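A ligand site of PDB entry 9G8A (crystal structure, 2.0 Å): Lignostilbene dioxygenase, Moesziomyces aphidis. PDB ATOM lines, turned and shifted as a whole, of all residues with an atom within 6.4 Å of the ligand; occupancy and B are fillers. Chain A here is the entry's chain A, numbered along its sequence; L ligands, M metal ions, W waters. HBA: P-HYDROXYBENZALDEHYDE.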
ATOM      1  N   LEU A  49      -1.690 -13.683 -11.022  1.00  0.00           N
ATOM      2  CA  LEU A  49      -1.917 -12.318 -10.558  1.00  0.00           C
ATOM      3  C   LEU A  49      -1.729 -12.128  -9.044  1.00  0.00           C
ATOM      4  O   LEU A  49      -1.292 -11.044  -8.633  1.00  0.00           O
ATOM      5  CB  LEU A  49      -3.190 -11.650 -11.105  1.00  0.00           C
ATOM      6  CG  LEU A  49      -3.151 -11.078 -12.534  1.00  0.00           C
ATOM      7  CD1 LEU A  49      -4.563 -10.636 -12.855  1.00  0.00           C
ATOM      8  CD2 LEU A  49      -2.213  -9.886 -12.739  1.00  0.00           C
ATOM      9  N   ILE A 102      -0.236 -12.692 -16.457  1.00  0.00           N
ATOM     10  CA  ILE A 102      -1.390 -12.684 -17.352  1.00  0.00           C
ATOM     11  C   ILE A 102      -1.178 -13.613 -18.562  1.00  0.00           C
ATOM     12  O   ILE A 102      -2.073 -13.708 -19.410  1.00  0.00           O
ATOM     13  CB  ILE A 102      -1.809 -11.241 -17.716  1.00  0.00           C
ATOM     14  CG1 ILE A 102      -0.703 -10.429 -18.470  1.00  0.00           C
ATOM     15  CG2 ILE A 102      -2.393 -10.501 -16.503  1.00  0.00           C
ATOM     16  CD1 ILE A 102      -1.166  -9.114 -19.107  1.00  0.00           C
ATOM     17  N   TYR A 144       4.398 -11.986 -23.903  1.00  0.00           N
ATOM     18  CA  TYR A 144       3.009 -11.560 -23.993  1.00  0.00           C
ATOM     19  C   TYR A 144       2.847 -10.690 -25.243  1.00  0.00           C
ATOM     20  O   TYR A 144       3.542  -9.679 -25.380  1.00  0.00           O
ATOM     21  CB  TYR A 144       2.569 -10.824 -22.730  1.00  0.00           C
ATOM     22  CG  TYR A 144       1.137 -10.301 -22.714  1.00  0.00           C
ATOM     23  CD1 TYR A 144       0.059 -11.159 -22.457  1.00  0.00           C
ATOM     24  CD2 TYR A 144       0.871  -8.941 -22.943  1.00  0.00           C
ATOM     25  CE1 TYR A 144      -1.248 -10.676 -22.441  1.00  0.00           C
ATOM     26  CE2 TYR A 144      -0.432  -8.433 -22.890  1.00  0.00           C
ATOM     27  CZ  TYR A 144      -1.491  -9.323 -22.668  1.00  0.00           C
ATOM     28  OH  TYR A 144      -2.774  -8.874 -22.642  1.00  0.00           O
ATOM     29  N   ARG A 145       2.014 -11.193 -26.177  1.00  0.00           N
ATOM     30  CA  ARG A 145       1.604 -10.492 -27.393  1.00  0.00           C
ATOM     31  C   ARG A 145       2.786 -10.108 -28.302  1.00  0.00           C
ATOM     32  O   ARG A 145       2.698  -9.124 -29.039  1.00  0.00           O
ATOM     33  CB  ARG A 145       0.658  -9.347 -27.008  1.00  0.00           C
ATOM     34  CG  ARG A 145      -0.648  -9.707 -26.311  1.00  0.00           C
ATOM     35  CD  ARG A 145      -1.526  -8.497 -26.291  1.00  0.00           C
ATOM     36  NE  ARG A 145      -2.122  -8.172 -27.603  1.00  0.00           N
ATOM     37  CZ  ARG A 145      -3.228  -7.465 -27.795  1.00  0.00           C
ATOM     38  NH1 ARG A 145      -3.906  -6.912 -26.782  1.00  0.00           N
ATOM     39  NH2 ARG A 145      -3.697  -7.355 -29.027  1.00  0.00           N
ATOM     40  N   ASN A 163      -7.547 -16.854 -21.386  1.00  0.00           N
ATOM     41  CA  ASN A 163      -7.317 -17.077 -19.948  1.00  0.00           C
ATOM     42  C   ASN A 163      -7.967 -16.038 -19.035  1.00  0.00           C
ATOM     43  O   ASN A 163      -7.727 -16.074 -17.822  1.00  0.00           O
ATOM     44  CB  ASN A 163      -5.815 -17.221 -19.659  1.00  0.00           C
ATOM     45  CG  ASN A 163      -4.989 -15.960 -19.787  1.00  0.00           C
ATOM     46  OD1 ASN A 163      -5.463 -14.894 -20.215  1.00  0.00           O
ATOM     47  ND2 ASN A 163      -3.721 -16.070 -19.424  1.00  0.00           N
ATOM     48  N   THR A 164      -8.763 -15.092 -19.602  1.00  0.00           N
ATOM     49  CA  THR A 164      -9.099 -13.850 -18.931  1.00  0.00           C
ATOM     50  C   THR A 164     -10.506 -13.884 -18.310  1.00  0.00           C
ATOM     51  O   THR A 164     -10.639 -13.537 -17.124  1.00  0.00           O
ATOM     52  CB  THR A 164      -8.870 -12.630 -19.819  1.00  0.00           C
ATOM     53  OG1 THR A 164      -7.529 -12.689 -20.306  1.00  0.00           O
ATOM     54  CG2 THR A 164      -9.066 -11.303 -19.099  1.00  0.00           C
ATOM     55  N   LYS A 177      -9.784 -13.814 -24.328  1.00  0.00           N
ATOM     56  CA  LYS A 177      -8.570 -13.046 -24.113  1.00  0.00           C
ATOM     57  C   LYS A 177      -8.458 -12.041 -25.252  1.00  0.00           C
ATOM     58  O   LYS A 177      -8.682 -12.411 -26.418  1.00  0.00           O
ATOM     59  CB  LYS A 177      -7.307 -13.916 -23.992  1.00  0.00           C
ATOM     60  CG  LYS A 177      -6.064 -13.204 -23.481  1.00  0.00           C
ATOM     61  CD  LYS A 177      -4.838 -14.123 -23.432  1.00  0.00           C
ATOM     62  CE  LYS A 177      -3.625 -13.429 -22.856  1.00  0.00           C
ATOM     63  NZ  LYS A 177      -3.812 -13.018 -21.449  1.00  0.00           N
ATOM     64  N   GLU A 178      -8.079 -10.804 -24.902  1.00  0.00           N
ATOM     65  CA  GLU A 178      -8.189  -9.606 -25.744  1.00  0.00           C
ATOM     66  C   GLU A 178      -7.350  -9.637 -27.029  1.00  0.00           C
ATOM     67  O   GLU A 178      -7.639  -8.816 -27.915  1.00  0.00           O
ATOM     68  CB  GLU A 178      -8.028  -8.276 -24.982  1.00  0.00           C
ATOM     69  CG  GLU A 178      -6.632  -8.016 -24.416  1.00  0.00           C
ATOM     70  CD  GLU A 178      -6.826  -7.151 -23.197  1.00  0.00           C
ATOM     71  OE1 GLU A 178      -7.272  -7.659 -22.123  1.00  0.00           O
ATOM     72  OE2 GLU A 178      -6.569  -5.954 -23.335  1.00  0.00           O
ATOM     73  N   ASN A 179      -6.347 -10.529 -27.136  1.00  0.00           N
ATOM     74  CA  ASN A 179      -5.450 -10.642 -28.289  1.00  0.00           C
ATOM     75  C   ASN A 179      -5.973 -11.616 -29.358  1.00  0.00           C
ATOM     76  O   ASN A 179      -5.256 -11.921 -30.321  1.00  0.00           O
ATOM     77  CB  ASN A 179      -4.007 -10.913 -27.859  1.00  0.00           C
ATOM     78  CG  ASN A 179      -3.814 -12.214 -27.116  1.00  0.00           C
ATOM     79  OD1 ASN A 179      -4.753 -12.732 -26.506  1.00  0.00           O
ATOM     80  ND2 ASN A 179      -2.596 -12.758 -27.120  1.00  0.00           N
ATOM     81  N   HIS A 208     -13.906  -8.321 -21.938  1.00  0.00           N
ATOM     82  CA  HIS A 208     -14.896  -7.584 -21.185  1.00  0.00           C
ATOM     83  C   HIS A 208     -16.093  -7.149 -22.030  1.00  0.00           C
ATOM     84  O   HIS A 208     -16.407  -5.957 -22.000  1.00  0.00           O
ATOM     85  CB  HIS A 208     -14.198  -6.463 -20.415  1.00  0.00           C
ATOM     86  CG  HIS A 208     -13.474  -6.982 -19.232  1.00  0.00           C
ATOM     87  ND1 HIS A 208     -14.117  -7.547 -18.166  1.00  0.00           N
ATOM     88  CD2 HIS A 208     -12.161  -7.045 -18.981  1.00  0.00           C
ATOM     89  CE1 HIS A 208     -13.216  -7.930 -17.292  1.00  0.00           C
ATOM     90  NE2 HIS A 208     -12.024  -7.645 -17.771  1.00  0.00           N
ATOM     91  N   PHE A 257      -3.892   0.142 -24.488  1.00  0.00           N
ATOM     92  CA  PHE A 257      -4.354  -1.068 -23.814  1.00  0.00           C
ATOM     93  C   PHE A 257      -5.778  -0.817 -23.331  1.00  0.00           C
ATOM     94  O   PHE A 257      -5.973  -0.237 -22.261  1.00  0.00           O
ATOM     95  CB  PHE A 257      -3.285  -1.370 -22.744  1.00  0.00           C
ATOM     96  CG  PHE A 257      -3.195  -2.759 -22.111  1.00  0.00           C
ATOM     97  CD1 PHE A 257      -4.312  -3.609 -21.986  1.00  0.00           C
ATOM     98  CD2 PHE A 257      -1.959  -3.185 -21.568  1.00  0.00           C
ATOM     99  CE1 PHE A 257      -4.196  -4.868 -21.389  1.00  0.00           C
ATOM    100  CE2 PHE A 257      -1.840  -4.455 -20.958  1.00  0.00           C
ATOM    101  CZ  PHE A 257      -2.948  -5.295 -20.874  1.00  0.00           C
ATOM    102  N   HIS A 259      -8.453  -2.617 -22.042  1.00  0.00           N
ATOM    103  CA  HIS A 259      -8.792  -3.856 -21.358  1.00  0.00           C
ATOM    104  C   HIS A 259     -10.299  -3.989 -21.096  1.00  0.00           C
ATOM    105  O   HIS A 259     -10.880  -5.064 -21.354  1.00  0.00           O
ATOM    106  CB  HIS A 259      -7.903  -4.012 -20.123  1.00  0.00           C
ATOM    107  CG  HIS A 259      -8.243  -5.234 -19.353  1.00  0.00           C
ATOM    108  ND1 HIS A 259      -8.019  -6.491 -19.879  1.00  0.00           N
ATOM    109  CD2 HIS A 259      -8.864  -5.429 -18.173  1.00  0.00           C
ATOM    110  CE1 HIS A 259      -8.462  -7.403 -19.035  1.00  0.00           C
ATOM    111  NE2 HIS A 259      -8.943  -6.770 -17.985  1.00  0.00           N
ATOM    112  N   TRP A 273      -5.986   2.461 -20.890  1.00  0.00           N
ATOM    113  CA  TRP A 273      -4.832   2.466 -19.998  1.00  0.00           C
ATOM    114  C   TRP A 273      -3.651   3.212 -20.643  1.00  0.00           C
ATOM    115  O   TRP A 273      -3.477   3.083 -21.862  1.00  0.00           O
ATOM    116  CB  TRP A 273      -4.415   1.055 -19.574  1.00  0.00           C
ATOM    117  CG  TRP A 273      -5.405   0.244 -18.782  1.00  0.00           C
ATOM    118  CD1 TRP A 273      -6.584   0.635 -18.200  1.00  0.00           C
ATOM    119  CD2 TRP A 273      -5.229  -1.151 -18.424  1.00  0.00           C
ATOM    120  NE1 TRP A 273      -7.179  -0.421 -17.564  1.00  0.00           N
ATOM    121  CE2 TRP A 273      -6.375  -1.528 -17.669  1.00  0.00           C
ATOM    122  CE3 TRP A 273      -4.231  -2.124 -18.664  1.00  0.00           C
ATOM    123  CZ2 TRP A 273      -6.526  -2.831 -17.144  1.00  0.00           C
ATOM    124  CZ3 TRP A 273      -4.375  -3.408 -18.147  1.00  0.00           C
ATOM    125  CH2 TRP A 273      -5.519  -3.744 -17.404  1.00  0.00           C
ATOM    126  N   ILE A 323      -8.260  -0.056 -13.594  1.00  0.00           N
ATOM    127  CA  ILE A 323      -8.051  -1.420 -14.084  1.00  0.00           C
ATOM    128  C   ILE A 323      -9.369  -1.972 -14.606  1.00  0.00           C
ATOM    129  O   ILE A 323      -9.428  -2.388 -15.766  1.00  0.00           O
ATOM    130  CB  ILE A 323      -7.313  -2.349 -13.100  1.00  0.00           C
ATOM    131  CG1 ILE A 323      -5.982  -1.731 -12.625  1.00  0.00           C
ATOM    132  CG2 ILE A 323      -7.119  -3.755 -13.685  1.00  0.00           C
ATOM    133  CD1 ILE A 323      -5.495  -2.276 -11.294  1.00  0.00           C
ATOM    134  N   HIS A 324     -10.409  -1.961 -13.745  1.00  0.00           N
ATOM    135  CA  HIS A 324     -11.716  -2.512 -14.034  1.00  0.00           C
ATOM    136  C   HIS A 324     -12.827  -1.545 -13.617  1.00  0.00           C
ATOM    137  O   HIS A 324     -12.740  -0.955 -12.540  1.00  0.00           O
ATOM    138  CB  HIS A 324     -11.901  -3.861 -13.333  1.00  0.00           C
ATOM    139  CG  HIS A 324     -11.093  -4.957 -13.918  1.00  0.00           C
ATOM    140  ND1 HIS A 324     -10.096  -5.595 -13.209  1.00  0.00           N
ATOM    141  CD2 HIS A 324     -11.167  -5.565 -15.108  1.00  0.00           C
ATOM    142  CE1 HIS A 324      -9.572  -6.533 -13.958  1.00  0.00           C
ATOM    143  NE2 HIS A 324     -10.204  -6.511 -15.126  1.00  0.00           N
ATOM    144  N   PHE A 348       0.828  -2.990 -13.450  1.00  0.00           N
ATOM    145  CA  PHE A 348       1.581  -4.015 -14.176  1.00  0.00           C
ATOM    146  C   PHE A 348       3.060  -3.606 -14.298  1.00  0.00           C
ATOM    147  O   PHE A 348       3.500  -3.381 -15.440  1.00  0.00           O
ATOM    148  CB  PHE A 348       0.858  -4.205 -15.528  1.00  0.00           C
ATOM    149  CG  PHE A 348      -0.409  -5.049 -15.676  1.00  0.00           C
ATOM    150  CD1 PHE A 348      -1.108  -5.573 -14.574  1.00  0.00           C
ATOM    151  CD2 PHE A 348      -0.906  -5.280 -16.972  1.00  0.00           C
ATOM    152  CE1 PHE A 348      -2.248  -6.373 -14.768  1.00  0.00           C
ATOM    153  CE2 PHE A 348      -2.072  -6.036 -17.167  1.00  0.00           C
ATOM    154  CZ  PHE A 348      -2.741  -6.588 -16.059  1.00  0.00           C
ATOM    155  N   GLU A 399     -10.196  -3.928  -6.329  1.00  0.00           N
ATOM    156  CA  GLU A 399     -10.072  -4.583  -7.619  1.00  0.00           C
ATOM    157  C   GLU A 399     -11.242  -5.532  -7.873  1.00  0.00           C
ATOM    158  O   GLU A 399     -12.125  -5.677  -7.028  1.00  0.00           O
ATOM    159  CB  GLU A 399      -8.680  -5.163  -7.918  1.00  0.00           C
ATOM    160  CG  GLU A 399      -7.964  -4.428  -9.052  1.00  0.00           C
ATOM    161  CD  GLU A 399      -8.757  -4.461 -10.347  1.00  0.00           C
ATOM    162  OE1 GLU A 399      -8.863  -5.558 -10.904  1.00  0.00           O
ATOM    163  OE2 GLU A 399      -9.370  -3.459 -10.752  1.00  0.00           O
ATOM    164  N   PHE A 400     -11.293  -6.078  -9.102  1.00  0.00           N
ATOM    165  CA  PHE A 400     -12.252  -7.079  -9.572  1.00  0.00           C
ATOM    166  C   PHE A 400     -13.685  -6.755  -9.117  1.00  0.00           C
ATOM    167  O   PHE A 400     -14.306  -7.602  -8.447  1.00  0.00           O
ATOM    168  CB  PHE A 400     -11.658  -8.446  -9.183  1.00  0.00           C
ATOM    169  CG  PHE A 400     -10.410  -8.919  -9.922  1.00  0.00           C
ATOM    170  CD1 PHE A 400     -10.471  -9.307 -11.269  1.00  0.00           C
ATOM    171  CD2 PHE A 400      -9.190  -9.088  -9.227  1.00  0.00           C
ATOM    172  CE1 PHE A 400      -9.340  -9.778 -11.955  1.00  0.00           C
ATOM    173  CE2 PHE A 400      -8.072  -9.585  -9.900  1.00  0.00           C
ATOM    174  CZ  PHE A 400      -8.139  -9.911 -11.261  1.00  0.00           C
ATOM    175  N   PHE A 432      -2.989  -6.516  -6.936  1.00  0.00           N
ATOM    176  CA  PHE A 432      -3.467  -7.865  -7.245  1.00  0.00           C
ATOM    177  C   PHE A 432      -3.090  -8.903  -6.182  1.00  0.00           C
ATOM    178  O   PHE A 432      -3.587 -10.032  -6.237  1.00  0.00           O
ATOM    179  CB  PHE A 432      -3.033  -8.294  -8.646  1.00  0.00           C
ATOM    180  CG  PHE A 432      -3.622  -7.487  -9.788  1.00  0.00           C
ATOM    181  CD1 PHE A 432      -4.940  -7.697 -10.221  1.00  0.00           C
ATOM    182  CD2 PHE A 432      -2.828  -6.525 -10.453  1.00  0.00           C
ATOM    183  CE1 PHE A 432      -5.467  -6.964 -11.281  1.00  0.00           C
ATOM    184  CE2 PHE A 432      -3.361  -5.784 -11.512  1.00  0.00           C
ATOM    185  CZ  PHE A 432      -4.676  -6.005 -11.933  1.00  0.00           C
ATOM    186  N   ILE A 517      -8.316 -14.943 -12.768  1.00  0.00           N
ATOM    187  CA  ILE A 517      -8.545 -13.593 -13.260  1.00  0.00           C
ATOM    188  C   ILE A 517     -10.033 -13.306 -13.018  1.00  0.00           C
ATOM    189  O   ILE A 517     -10.386 -12.912 -11.893  1.00  0.00           O
ATOM    190  CB  ILE A 517      -7.952 -13.371 -14.684  1.00  0.00           C
ATOM    191  CG1 ILE A 517      -6.457 -13.846 -14.787  1.00  0.00           C
ATOM    192  CG2 ILE A 517      -8.104 -11.900 -15.085  1.00  0.00           C
ATOM    193  CD1 ILE A 517      -5.767 -13.733 -16.146  1.00  0.00           C
ATOM    194  N   HIS A 518     -10.891 -13.590 -14.012  1.00  0.00           N
ATOM    195  CA  HIS A 518     -12.336 -13.414 -13.873  1.00  0.00           C
ATOM    196  C   HIS A 518     -13.038 -14.746 -13.702  1.00  0.00           C
ATOM    197  O   HIS A 518     -12.517 -15.798 -14.101  1.00  0.00           O
ATOM    198  CB  HIS A 518     -12.946 -12.573 -15.003  1.00  0.00           C
ATOM    199  CG  HIS A 518     -12.428 -11.190 -14.982  1.00  0.00           C
ATOM    200  ND1 HIS A 518     -12.849 -10.206 -14.112  1.00  0.00           N
ATOM    201  CD2 HIS A 518     -11.448 -10.667 -15.702  1.00  0.00           C
ATOM    202  CE1 HIS A 518     -12.148  -9.105 -14.321  1.00  0.00           C
ATOM    203  NE2 HIS A 518     -11.272  -9.371 -15.265  1.00  0.00           N
HETATM  204  C1' HBA L   1      -6.012  -7.782 -16.441  1.00  0.00           C
HETATM  205  O1' HBA L   1      -6.655  -8.245 -15.505  1.00  0.00           O
HETATM  206  C1  HBA L   1      -5.588  -8.511 -17.653  1.00  0.00           C
HETATM  207  C2  HBA L   1      -5.797  -9.887 -17.805  1.00  0.00           C
HETATM  208  C3  HBA L   1      -5.411 -10.562 -18.959  1.00  0.00           C
HETATM  209  C4  HBA L   1      -4.843  -9.827 -20.003  1.00  0.00           C
HETATM  210  C5  HBA L   1      -4.677  -8.442 -19.902  1.00  0.00           C
HETATM  211  C6  HBA L   1      -5.037  -7.786 -18.732  1.00  0.00           C
HETATM  212  O4  HBA L   1      -4.490 -10.448 -21.179  1.00  0.00           O
HETATM  213 FE    FE M   1     -10.153  -8.053 -16.592  1.00  0.00          FE
HETATM  214  O   HOH W   1      -8.813  -9.266 -16.559  1.00  0.00           O
HETATM  215  O   HOH W   2      -7.581 -10.376 -22.135  1.00  0.00           O
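The side-chain hydroxyl (OH) of Tyr 144 is in hydrogen-bond range of an oxygen (O4) of the ligand (2.8 Å).
An oxygen (O4) of the ligand lies within hydrogen-bond range of the side-chain amino group (NZ) of Lys 177 (2.7 Å).
The backbone carbonyl oxygen (O) of Ile 102 is in hydrogen-bond range of the side-chain amide nitrogen (ND2) of Asn 163.
The backbone NH of His 518 lies within hydrogen-bond range of the backbone carbonyl oxygen of Thr 164.
The backbone carbonyl oxygen (O) of Phe 257 lies within hydrogen-bond range of the backbone NH (N) of Trp 273, 3.0 Å away.
A ring nitrogen (ND1) of His 259 lies within hydrogen-bond range of the side-chain carboxylate (OE1) of Glu 178 (2.6 Å).
NZ of Lys 177 lies within hydrogen-bond range of O of Ile 102.
OE1 of Glu 399 lies within hydrogen-bond range of ND1 of His 324, 2.6 Å away.
The side-chain amino group (NZ) of Lys 177 sits at hydrogen-bond distance from the side-chain amide oxygen (OD1) of Asn 163.
The side-chain amide oxygen (OD1) of Asn 163 lies within hydrogen-bond range of the side-chain hydroxyl (OG1) of Thr 164 (3.0 Å).
Merely in contact with the ligand: Thr 164 (3.3 Å), His 259 (3.4 Å), Phe 348 (3.5 Å), Glu 178 (3.5 Å), Ile 102 (3.7 Å), His 324 (3.7 Å), Phe 257 (3.7 Å) and Ile 517 (3.95 Å).
Hydrophobic or aromatic side chains that line the ligand: Ile 102, Tyr 144, Phe 257, His 259, His 324, Phe 348 and Ile 517.
Within 4 Å of the ligand: Ile 102, Tyr 144, Thr 164, Lys 177, Glu 178, Phe 257, His 259, His 324, Phe 348 and Ile 517.
Water W2 lies within hydrogen-bond range of OE1 of Glu 178 (2.7 Å), OG1 of Thr 164 (2.9 Å) and O4 of the ligand (3.2 Å).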
